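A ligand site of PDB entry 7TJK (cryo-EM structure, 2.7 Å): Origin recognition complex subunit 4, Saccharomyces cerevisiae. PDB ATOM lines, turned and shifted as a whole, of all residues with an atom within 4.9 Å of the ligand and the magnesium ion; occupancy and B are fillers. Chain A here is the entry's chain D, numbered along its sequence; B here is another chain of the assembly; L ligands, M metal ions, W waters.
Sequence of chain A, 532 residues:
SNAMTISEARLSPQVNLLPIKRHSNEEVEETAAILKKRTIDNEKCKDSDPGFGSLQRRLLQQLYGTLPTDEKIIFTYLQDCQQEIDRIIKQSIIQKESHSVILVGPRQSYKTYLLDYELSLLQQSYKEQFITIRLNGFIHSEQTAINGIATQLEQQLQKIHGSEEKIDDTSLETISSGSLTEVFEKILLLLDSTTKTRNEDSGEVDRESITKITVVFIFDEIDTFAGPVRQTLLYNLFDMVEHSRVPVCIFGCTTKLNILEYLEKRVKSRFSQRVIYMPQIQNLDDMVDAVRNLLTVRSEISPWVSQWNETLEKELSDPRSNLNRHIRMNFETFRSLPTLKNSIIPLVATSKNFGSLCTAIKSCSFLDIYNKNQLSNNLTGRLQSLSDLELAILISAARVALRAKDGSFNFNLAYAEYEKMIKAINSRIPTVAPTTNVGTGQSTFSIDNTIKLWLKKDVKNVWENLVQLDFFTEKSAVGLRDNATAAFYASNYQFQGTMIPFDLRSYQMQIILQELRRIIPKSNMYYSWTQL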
ATOM      1  N   TYR A  64     -32.601  11.335 -10.144  1.00  0.00           N
ATOM      2  CA  TYR A  64     -32.934   9.914 -10.085  1.00  0.00           C
ATOM      3  C   TYR A  64     -31.850   9.031 -10.693  1.00  0.00           C
ATOM      4  O   TYR A  64     -31.982   7.808 -10.664  1.00  0.00           O
ATOM      5  CB  TYR A  64     -34.265   9.638 -10.805  1.00  0.00           C
ATOM      6  CG  TYR A  64     -35.494   9.998  -9.993  1.00  0.00           C
ATOM      7  CD1 TYR A  64     -36.011   9.119  -9.047  1.00  0.00           C
ATOM      8  CD2 TYR A  64     -36.149  11.204 -10.187  1.00  0.00           C
ATOM      9  CE1 TYR A  64     -37.139   9.447  -8.301  1.00  0.00           C
ATOM     10  CE2 TYR A  64     -37.263  11.545  -9.452  1.00  0.00           C
ATOM     11  CZ  TYR A  64     -37.762  10.661  -8.517  1.00  0.00           C
ATOM     12  OH  TYR A  64     -38.874  11.004  -7.795  1.00  0.00           O
ATOM     13  N   GLY A  65     -30.790   9.628 -11.233  1.00  0.00           N
ATOM     14  CA  GLY A  65     -29.660   8.865 -11.729  1.00  0.00           C
ATOM     15  C   GLY A  65     -29.928   8.060 -12.979  1.00  0.00           C
ATOM     16  O   GLY A  65     -29.203   7.101 -13.256  1.00  0.00           O
ATOM     17  N   THR A  66     -30.942   8.426 -13.757  1.00  0.00           N
ATOM     18  CA  THR A  66     -31.367   7.648 -14.914  1.00  0.00           C
ATOM     19  C   THR A  66     -30.885   8.256 -16.228  1.00  0.00           C
ATOM     20  O   THR A  66     -31.589   8.195 -17.238  1.00  0.00           O
ATOM     21  CB  THR A  66     -32.886   7.507 -14.912  1.00  0.00           C
ATOM     22  OG1 THR A  66     -33.486   8.776 -14.638  1.00  0.00           O
ATOM     23  CG2 THR A  66     -33.332   6.506 -13.864  1.00  0.00           C
ATOM     24  N   LYS A  72     -23.516   9.408 -17.107  1.00  0.00           N
ATOM     25  CA  LYS A  72     -23.924   9.095 -15.747  1.00  0.00           C
ATOM     26  C   LYS A  72     -22.930   9.665 -14.747  1.00  0.00           C
ATOM     27  O   LYS A  72     -21.729   9.768 -15.026  1.00  0.00           O
ATOM     28  CB  LYS A  72     -24.044   7.570 -15.613  1.00  0.00           C
ATOM     29  CG  LYS A  72     -24.816   7.079 -14.407  1.00  0.00           C
ATOM     30  CD  LYS A  72     -25.026   5.572 -14.495  1.00  0.00           C
ATOM     31  CE  LYS A  72     -25.777   5.055 -13.288  1.00  0.00           C
ATOM     32  NZ  LYS A  72     -25.936   3.567 -13.279  1.00  0.00           N
ATOM     33  N   PRO A 106     -22.958   0.115   3.912  1.00  0.00           N
ATOM     34  CA  PRO A 106     -24.333   0.257   4.401  1.00  0.00           C
ATOM     35  C   PRO A 106     -25.377   0.269   3.300  1.00  0.00           C
ATOM     36  O   PRO A 106     -25.052   0.191   2.109  1.00  0.00           O
ATOM     37  CB  PRO A 106     -24.307   1.603   5.149  1.00  0.00           C
ATOM     38  CG  PRO A 106     -23.101   2.296   4.656  1.00  0.00           C
ATOM     39  CD  PRO A 106     -22.108   1.254   4.314  1.00  0.00           C
ATOM     40  N   ARG A 107     -26.653   0.327   3.682  1.00  0.00           N
ATOM     41  CA  ARG A 107     -27.699   0.498   2.695  1.00  0.00           C
ATOM     42  C   ARG A 107     -27.613   1.872   2.068  1.00  0.00           C
ATOM     43  O   ARG A 107     -27.210   2.844   2.714  1.00  0.00           O
ATOM     44  CB  ARG A 107     -29.080   0.291   3.332  1.00  0.00           C
ATOM     45  CG  ARG A 107     -29.255  -1.066   3.982  1.00  0.00           C
ATOM     46  CD  ARG A 107     -30.674  -1.567   3.840  1.00  0.00           C
ATOM     47  NE  ARG A 107     -30.775  -2.982   4.166  1.00  0.00           N
ATOM     48  CZ  ARG A 107     -30.644  -3.972   3.288  1.00  0.00           C
ATOM     49  NH1 ARG A 107     -30.412  -3.729   2.010  1.00  0.00           N
ATOM     50  NH2 ARG A 107     -30.758  -5.230   3.713  1.00  0.00           N
ATOM     51  N   GLN A 108     -27.963   1.936   0.773  1.00  0.00           N
ATOM     52  CA  GLN A 108     -27.903   3.148  -0.059  1.00  0.00           C
ATOM     53  C   GLN A 108     -26.488   3.720  -0.120  1.00  0.00           C
ATOM     54  O   GLN A 108     -26.292   4.935  -0.082  1.00  0.00           O
ATOM     55  CB  GLN A 108     -28.908   4.202   0.411  1.00  0.00           C
ATOM     56  CG  GLN A 108     -30.352   3.716   0.467  1.00  0.00           C
ATOM     57  CD  GLN A 108     -30.916   3.418  -0.901  1.00  0.00           C
ATOM     58  OE1 GLN A 108     -31.272   4.334  -1.654  1.00  0.00           O
ATOM     59  NE2 GLN A 108     -31.019   2.137  -1.238  1.00  0.00           N
ATOM     60  N   SER A 109     -25.491   2.843  -0.216  1.00  0.00           N
ATOM     61  CA  SER A 109     -24.091   3.247  -0.329  1.00  0.00           C
ATOM     62  C   SER A 109     -23.527   2.982  -1.722  1.00  0.00           C
ATOM     63  O   SER A 109     -22.313   2.771  -1.847  1.00  0.00           O
ATOM     64  CB  SER A 109     -23.242   2.557   0.738  1.00  0.00           C
ATOM     65  OG  SER A 109     -23.216   1.157   0.548  1.00  0.00           O
ATOM     66  N   TYR A 110     -24.391   2.942  -2.734  1.00  0.00           N
ATOM     67  CA  TYR A 110     -24.038   2.892  -4.155  1.00  0.00           C
ATOM     68  C   TYR A 110     -23.308   1.610  -4.553  1.00  0.00           C
ATOM     69  O   TYR A 110     -22.432   1.626  -5.403  1.00  0.00           O
ATOM     70  CB  TYR A 110     -23.224   4.133  -4.584  1.00  0.00           C
ATOM     71  CG  TYR A 110     -23.965   5.433  -4.387  1.00  0.00           C
ATOM     72  CD1 TYR A 110     -23.870   6.135  -3.189  1.00  0.00           C
ATOM     73  CD2 TYR A 110     -24.762   5.958  -5.396  1.00  0.00           C
ATOM     74  CE1 TYR A 110     -24.552   7.326  -3.007  1.00  0.00           C
ATOM     75  CE2 TYR A 110     -25.442   7.139  -5.215  1.00  0.00           C
ATOM     76  CZ  TYR A 110     -25.334   7.824  -4.023  1.00  0.00           C
ATOM     77  OH  TYR A 110     -26.006   9.008  -3.847  1.00  0.00           O
ATOM     78  N   LYS A 111     -23.675   0.485  -3.934  1.00  0.00           N
ATOM     79  CA  LYS A 111     -23.136  -0.803  -4.371  1.00  0.00           C
ATOM     80  C   LYS A 111     -23.816  -1.269  -5.650  1.00  0.00           C
ATOM     81  O   LYS A 111     -23.140  -1.556  -6.652  1.00  0.00           O
ATOM     82  CB  LYS A 111     -23.309  -1.850  -3.261  1.00  0.00           C
ATOM     83  CG  LYS A 111     -22.593  -1.511  -1.966  1.00  0.00           C
ATOM     84  CD  LYS A 111     -22.571  -2.697  -1.010  1.00  0.00           C
ATOM     85  CE  LYS A 111     -23.952  -3.063  -0.524  1.00  0.00           C
ATOM     86  NZ  LYS A 111     -24.573  -1.989   0.290  1.00  0.00           N
ATOM     87  N   THR A 112     -25.148  -1.342  -5.626  1.00  0.00           N
ATOM     88  CA  THR A 112     -25.937  -1.686  -6.796  1.00  0.00           C
ATOM     89  C   THR A 112     -25.775  -0.652  -7.909  1.00  0.00           C
ATOM     90  O   THR A 112     -25.720  -1.027  -9.083  1.00  0.00           O
ATOM     91  CB  THR A 112     -27.413  -1.825  -6.384  1.00  0.00           C
ATOM     92  OG1 THR A 112     -27.530  -2.842  -5.378  1.00  0.00           O
ATOM     93  CG2 THR A 112     -28.319  -2.157  -7.537  1.00  0.00           C
ATOM     94  N   TYR A 113     -25.664   0.630  -7.541  1.00  0.00           N
ATOM     95  CA  TYR A 113     -25.443   1.703  -8.504  1.00  0.00           C
ATOM     96  C   TYR A 113     -24.143   1.503  -9.276  1.00  0.00           C
ATOM     97  O   TYR A 113     -24.130   1.554 -10.513  1.00  0.00           O
ATOM     98  CB  TYR A 113     -25.436   3.045  -7.766  1.00  0.00           C
ATOM     99  CG  TYR A 113     -25.259   4.277  -8.622  1.00  0.00           C
ATOM    100  CD1 TYR A 113     -26.351   4.932  -9.164  1.00  0.00           C
ATOM    101  CD2 TYR A 113     -23.989   4.820  -8.859  1.00  0.00           C
ATOM    102  CE1 TYR A 113     -26.197   6.072  -9.930  1.00  0.00           C
ATOM    103  CE2 TYR A 113     -23.828   5.941  -9.640  1.00  0.00           C
ATOM    104  CZ  TYR A 113     -24.938   6.570 -10.166  1.00  0.00           C
ATOM    105  OH  TYR A 113     -24.772   7.692 -10.939  1.00  0.00           O
ATOM    106  N   ASP A 116     -24.322  -1.755 -11.503  1.00  0.00           N
ATOM    107  CA  ASP A 116     -25.096  -1.555 -12.717  1.00  0.00           C
ATOM    108  C   ASP A 116     -24.397  -0.618 -13.687  1.00  0.00           C
ATOM    109  O   ASP A 116     -24.489  -0.812 -14.905  1.00  0.00           O
ATOM    110  CB  ASP A 116     -26.493  -1.018 -12.398  1.00  0.00           C
ATOM    111  CG  ASP A 116     -27.429  -2.078 -11.873  1.00  0.00           C
ATOM    112  OD1 ASP A 116     -27.619  -3.096 -12.575  1.00  0.00           O
ATOM    113  OD2 ASP A 116     -27.956  -1.903 -10.763  1.00  0.00           O
ATOM    114  N   ASP A 220     -26.786 -10.270  -4.208  1.00  0.00           N
ATOM    115  CA  ASP A 220     -27.108  -9.338  -3.143  1.00  0.00           C
ATOM    116  C   ASP A 220     -27.585 -10.066  -1.889  1.00  0.00           C
ATOM    117  O   ASP A 220     -28.199 -11.139  -1.974  1.00  0.00           O
ATOM    118  CB  ASP A 220     -28.190  -8.364  -3.598  1.00  0.00           C
ATOM    119  CG  ASP A 220     -27.734  -7.501  -4.757  1.00  0.00           C
ATOM    120  OD1 ASP A 220     -26.649  -6.897  -4.666  1.00  0.00           O
ATOM    121  OD2 ASP A 220     -28.475  -7.436  -5.769  1.00  0.00           O
ATOM    122  N   GLU A 221     -27.337  -9.437  -0.737  1.00  0.00           N
ATOM    123  CA  GLU A 221     -27.531 -10.024   0.597  1.00  0.00           C
ATOM    124  C   GLU A 221     -26.860 -11.387   0.714  1.00  0.00           C
ATOM    125  O   GLU A 221     -27.503 -12.410   0.959  1.00  0.00           O
ATOM    126  CB  GLU A 221     -29.014 -10.091   0.992  1.00  0.00           C
ATOM    127  CG  GLU A 221     -29.913  -8.983   0.442  1.00  0.00           C
ATOM    128  CD  GLU A 221     -29.754  -7.665   1.187  1.00  0.00           C
ATOM    129  OE1 GLU A 221     -29.111  -7.644   2.256  1.00  0.00           O
ATOM    130  OE2 GLU A 221     -30.288  -6.643   0.702  1.00  0.00           O
ATOM    131  N   THR A 255     -24.167  -5.710   4.083  1.00  0.00           N
ATOM    132  CA  THR A 255     -23.990  -4.549   4.982  1.00  0.00           C
ATOM    133  C   THR A 255     -23.151  -5.021   6.176  1.00  0.00           C
ATOM    134  O   THR A 255     -22.650  -4.141   6.901  1.00  0.00           O
ATOM    135  CB  THR A 255     -25.358  -4.000   5.415  1.00  0.00           C
ATOM    136  OG1 THR A 255     -26.052  -5.055   6.066  1.00  0.00           O
ATOM    137  CG2 THR A 255     -26.195  -3.498   4.253  1.00  0.00           C
ATOM    138  N   PRO A 338     -28.887  10.005  -0.722  1.00  0.00           N
ATOM    139  CA  PRO A 338     -30.304   9.697  -1.012  1.00  0.00           C
ATOM    140  C   PRO A 338     -31.301  10.391  -0.098  1.00  0.00           C
ATOM    141  O   PRO A 338     -32.393  10.754  -0.565  1.00  0.00           O
ATOM    142  CB  PRO A 338     -30.359   8.177  -0.839  1.00  0.00           C
ATOM    143  CG  PRO A 338     -29.049   7.725  -1.243  1.00  0.00           C
ATOM    144  CD  PRO A 338     -28.083   8.756  -0.760  1.00  0.00           C
ATOM    145  N   LYS A 341     -31.540  13.795  -1.498  1.00  0.00           N
ATOM    146  CA  LYS A 341     -32.195  13.730  -2.809  1.00  0.00           C
ATOM    147  C   LYS A 341     -33.696  13.578  -2.683  1.00  0.00           C
ATOM    148  O   LYS A 341     -34.448  14.157  -3.486  1.00  0.00           O
ATOM    149  CB  LYS A 341     -31.620  12.572  -3.617  1.00  0.00           C
ATOM    150  CG  LYS A 341     -30.397  12.934  -4.445  1.00  0.00           C
ATOM    151  CD  LYS A 341     -29.547  11.712  -4.811  1.00  0.00           C
ATOM    152  CE  LYS A 341     -30.377  10.505  -5.194  1.00  0.00           C
ATOM    153  NZ  LYS A 341     -29.515   9.323  -5.476  1.00  0.00           N
ATOM    154  N   LYS B 151     -36.816  -4.651  -3.155  1.00  0.00           N
ATOM    155  CA  LYS B 151     -35.830  -5.076  -4.134  1.00  0.00           C
ATOM    156  C   LYS B 151     -36.429  -5.814  -5.323  1.00  0.00           C
ATOM    157  O   LYS B 151     -35.683  -6.445  -6.085  1.00  0.00           O
ATOM    158  CB  LYS B 151     -34.773  -5.953  -3.466  1.00  0.00           C
ATOM    159  CG  LYS B 151     -33.933  -5.250  -2.413  1.00  0.00           C
ATOM    160  CD  LYS B 151     -33.220  -4.039  -2.976  1.00  0.00           C
ATOM    161  CE  LYS B 151     -32.454  -3.304  -1.890  1.00  0.00           C
ATOM    162  NZ  LYS B 151     -31.813  -2.063  -2.382  1.00  0.00           N
ATOM    163  N   GLU B 154     -35.365  -4.679  -8.963  1.00  0.00           N
ATOM    164  CA  GLU B 154     -34.004  -4.984  -9.360  1.00  0.00           C
ATOM    165  C   GLU B 154     -33.890  -6.338 -10.057  1.00  0.00           C
ATOM    166  O   GLU B 154     -32.968  -6.540 -10.862  1.00  0.00           O
ATOM    167  CB  GLU B 154     -33.119  -4.909  -8.111  1.00  0.00           C
ATOM    168  CG  GLU B 154     -32.919  -3.555  -7.472  1.00  0.00           C
ATOM    169  CD  GLU B 154     -32.090  -3.629  -6.202  1.00  0.00           C
ATOM    170  OE1 GLU B 154     -31.822  -4.761  -5.726  1.00  0.00           O
ATOM    171  OE2 GLU B 154     -31.689  -2.569  -5.699  1.00  0.00           O
ATOM    172  N   LYS B 158     -34.347  -3.983 -16.947  1.00  0.00           N
ATOM    173  CA  LYS B 158     -34.245  -2.520 -16.975  1.00  0.00           C
ATOM    174  C   LYS B 158     -34.799  -1.929 -18.270  1.00  0.00           C
ATOM    175  O   LYS B 158     -35.409  -0.857 -18.245  1.00  0.00           O
ATOM    176  CB  LYS B 158     -32.779  -2.113 -16.768  1.00  0.00           C
ATOM    177  CG  LYS B 158     -32.507  -0.607 -16.772  1.00  0.00           C
ATOM    178  CD  LYS B 158     -33.120   0.079 -15.559  1.00  0.00           C
ATOM    179  CE  LYS B 158     -32.302  -0.205 -14.303  1.00  0.00           C
ATOM    180  NZ  LYS B 158     -32.778   0.590 -13.137  1.00  0.00           N
ATOM    181  N   HIS B 182     -33.393   2.371   3.958  1.00  0.00           N
ATOM    182  CA  HIS B 182     -33.637   2.158   2.541  1.00  0.00           C
ATOM    183  C   HIS B 182     -33.862   3.469   1.793  1.00  0.00           C
ATOM    184  O   HIS B 182     -33.726   3.468   0.564  1.00  0.00           O
ATOM    185  CB  HIS B 182     -34.848   1.248   2.345  1.00  0.00           C
ATOM    186  CG  HIS B 182     -34.552  -0.206   2.574  1.00  0.00           C
ATOM    187  ND1 HIS B 182     -33.850  -0.977   1.678  1.00  0.00           N
ATOM    188  CD2 HIS B 182     -34.859  -1.015   3.611  1.00  0.00           C
ATOM    189  CE1 HIS B 182     -33.751  -2.203   2.147  1.00  0.00           C
ATOM    190  NE2 HIS B 182     -34.344  -2.254   3.319  1.00  0.00           N
HETATM  191  P1  LIG L   1     -28.555  -1.848  -0.416  1.00  0.00           P
HETATM  192  O1  LIG L   1     -27.578  -2.236   0.634  1.00  0.00           O
HETATM  193  O2  LIG L   1     -28.792  -2.946  -1.442  1.00  0.00           O
HETATM  194  O3  LIG L   1     -29.890  -1.368   0.123  1.00  0.00           O
HETATM  195  P2  LIG L   1     -26.772  -0.225  -2.173  1.00  0.00           P
HETATM  196  O4  LIG L   1     -26.556  -1.226  -3.218  1.00  0.00           O
HETATM  197  O5  LIG L   1     -25.607   0.061  -1.241  1.00  0.00           O
HETATM  198  O6  LIG L   1     -28.009  -0.615  -1.270  1.00  0.00           O
HETATM  199  P3  LIG L   1     -27.695   1.730  -4.183  1.00  0.00           P
HETATM  200  O7  LIG L   1     -29.114   1.411  -4.447  1.00  0.00           O
HETATM  201  O8  LIG L   1     -26.721   1.181  -5.211  1.00  0.00           O
HETATM  202  O9  LIG L   1     -27.237   1.172  -2.779  1.00  0.00           O
HETATM  203  O10 LIG L   1     -27.436   3.281  -4.099  1.00  0.00           O
HETATM  204  C1  LIG L   1     -28.436   4.178  -3.563  1.00  0.00           C
HETATM  205  C2  LIG L   1     -28.804   5.207  -4.602  1.00  0.00           C
HETATM  206  O11 LIG L   1     -28.480   4.721  -5.923  1.00  0.00           O
HETATM  207  C3  LIG L   1     -30.299   5.559  -4.632  1.00  0.00           C
HETATM  208  O12 LIG L   1     -30.484   6.948  -4.856  1.00  0.00           O
HETATM  209  C4  LIG L   1     -30.817   4.706  -5.789  1.00  0.00           C
HETATM  210  O13 LIG L   1     -31.979   5.274  -6.393  1.00  0.00           O
HETATM  211  C5  LIG L   1     -29.628   4.766  -6.750  1.00  0.00           C
HETATM  212  N1  LIG L   1     -29.557   3.661  -7.706  1.00  0.00           N
HETATM  213  C6  LIG L   1     -29.440   2.325  -7.431  1.00  0.00           C
HETATM  214  N2  LIG L   1     -29.393   1.570  -8.489  1.00  0.00           N
HETATM  215  C7  LIG L   1     -29.488   2.462  -9.540  1.00  0.00           C
HETATM  216  C8  LIG L   1     -29.495   2.299 -10.943  1.00  0.00           C
HETATM  217  N3  LIG L   1     -29.409   1.109 -11.544  1.00  0.00           N
HETATM  218  N4  LIG L   1     -29.599   3.404 -11.711  1.00  0.00           N
HETATM  219  C9  LIG L   1     -29.691   4.592 -11.118  1.00  0.00           C
HETATM  220  N5  LIG L   1     -29.695   4.871  -9.807  1.00  0.00           N
HETATM  221  C10 LIG L   1     -29.590   3.758  -9.076  1.00  0.00           C
HETATM  222 MG    MG M   1     -28.318  -3.111  -3.494  1.00  0.00          MG
HETATM  223  O   HOH W   1     -32.838   8.590  -3.788  1.00  0.00           O
HETATM  224  O   HOH W   2     -26.381  -4.169  -2.981  1.00  0.00           O
HETATM  225  O   HOH W   3     -29.933  -1.474  -4.034  1.00  0.00           O
HETATM  226  O   HOH W   4     -32.720   7.815  -7.116  1.00  0.00           O
HETATM  227  O   HOH W   5     -31.622   0.357   0.385  1.00  0.00           O
HETATM  228  O   HOH W   6     -31.946   1.375  -4.164  1.00  0.00           O
HETATM  229  O   HOH W   7     -29.735  -4.932  -3.918  1.00  0.00           O
HETATM  230  O   HOH W   8     -30.217  -5.864  -1.633  1.00  0.00           O
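The backbone NH (N) of Thr 112 is in hydrogen-bond range of an oxygen (O8) of the ligand, 3.0 Å away.
An oxygen (O8) of the ligand sits at hydrogen-bond distance from the backbone NH (N) of Tyr 113, at 2.6 Å.
NZ of Lys 341 sits at hydrogen-bond distance from O12 of the ligand (2.6 Å).
The backbone NH of Lys 111 is in hydrogen-bond range of an oxygen (O5) of the ligand (3.3 Å).
An oxygen (O5) of the ligand lies within salt-bridge range of the side-chain amino group of Lys 111.
The backbone NH (N) of Ser 109 is in hydrogen-bond range of an oxygen (O5) of the ligand (3.0 Å).
O5 of the ligand sits at hydrogen-bond distance from OG of Ser 109, at 3.2 Å.
NH1 of Arg 107 is in salt-bridge range of O3 of the ligand, 3.1 Å away.
The side-chain amino group of Lys 151 of chain B is in salt-bridge range of an oxygen (O3) of the ligand.
An oxygen (O6) of the ligand is in hydrogen-bond range of the backbone NH (N) of Gln 108, 3.3 Å away.
An oxygen (O9) of the ligand is in hydrogen-bond range of the backbone NH (N) of Tyr 110.
The side-chain carboxylate (OD2) of Asp 116 sits at hydrogen-bond distance from a nitrogen (N3) of the ligand (3.4 Å).
The side-chain amino group (NZ) of Lys 111 sits at hydrogen-bond distance from the side-chain hydroxyl (OG) of Ser 109 (3.4 Å).
The backbone carbonyl oxygen (O) of Pro 106 lies within hydrogen-bond range of the side-chain amino group (NZ) of Lys 111 (2.9 Å).
OG of Ser 109 is in hydrogen-bond range of O of Pro 106.
NH1 of Arg 107 lies within salt-bridge range of OE2 of Glu 221, 3.2 Å away.
The side-chain amino group (NZ) of Lys 151 of chain B lies within salt-bridge range of the side-chain carboxylate (OE2) of Glu 154 of chain B (3.4 Å).
The side-chain amide oxygen (OE1) of Gln 108 sits close to the backbone carbonyl oxygen (O) of His 182 of chain B.
O of Pro 106 sits close to O5 of the ligand (3.4 Å).
Tyr 64 touches the ligand.
Gly 65 touches the ligand.
Lys 72 touches the ligand.
CG of Pro 338 touches O12 of the ligand, 3.96 Å away.
Lys 158 of chain B touches the ligand.
Hydrophobic or aromatic side chains that line the ligand: Tyr 110, Tyr 113 and Pro 338.
Lys 151 of chain B touches the magnesium ion.
Of the 22 residues printed, 2 come within 4 Å of the magnesium ion.
The nearest printed residue that does not touch the magnesium ion is Glu 154 of chain B (4.1 Å).
The magnesium ion is bound by the side-chain hydroxyl of Thr 112, an oxygen (O2) of the ligand, water W2, water W7, water W3 and an oxygen (O4) of the ligand.
The magnesium ion has six donor atoms within binding distance.
Water W7 bridges OE1 of Glu 154 of chain B and OD2 of Asp 220.
Water W3 lies within hydrogen-bond range of NZ of Lys 151 of chain B, OE2 of Glu 154 of chain B and O7 of the ligand.
Water W5 lies within hydrogen-bond range of an oxygen (O3) of the ligand (2.5 Å), the side-chain amide nitrogen of Gln 108 (2.5 Å) and a ring nitrogen (ND1) of His 182 of chain B (2.9 Å).
Water W6 bridges O7 of the ligand (2.8 Å) and NE2 of Gln 108 (3.2 Å).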
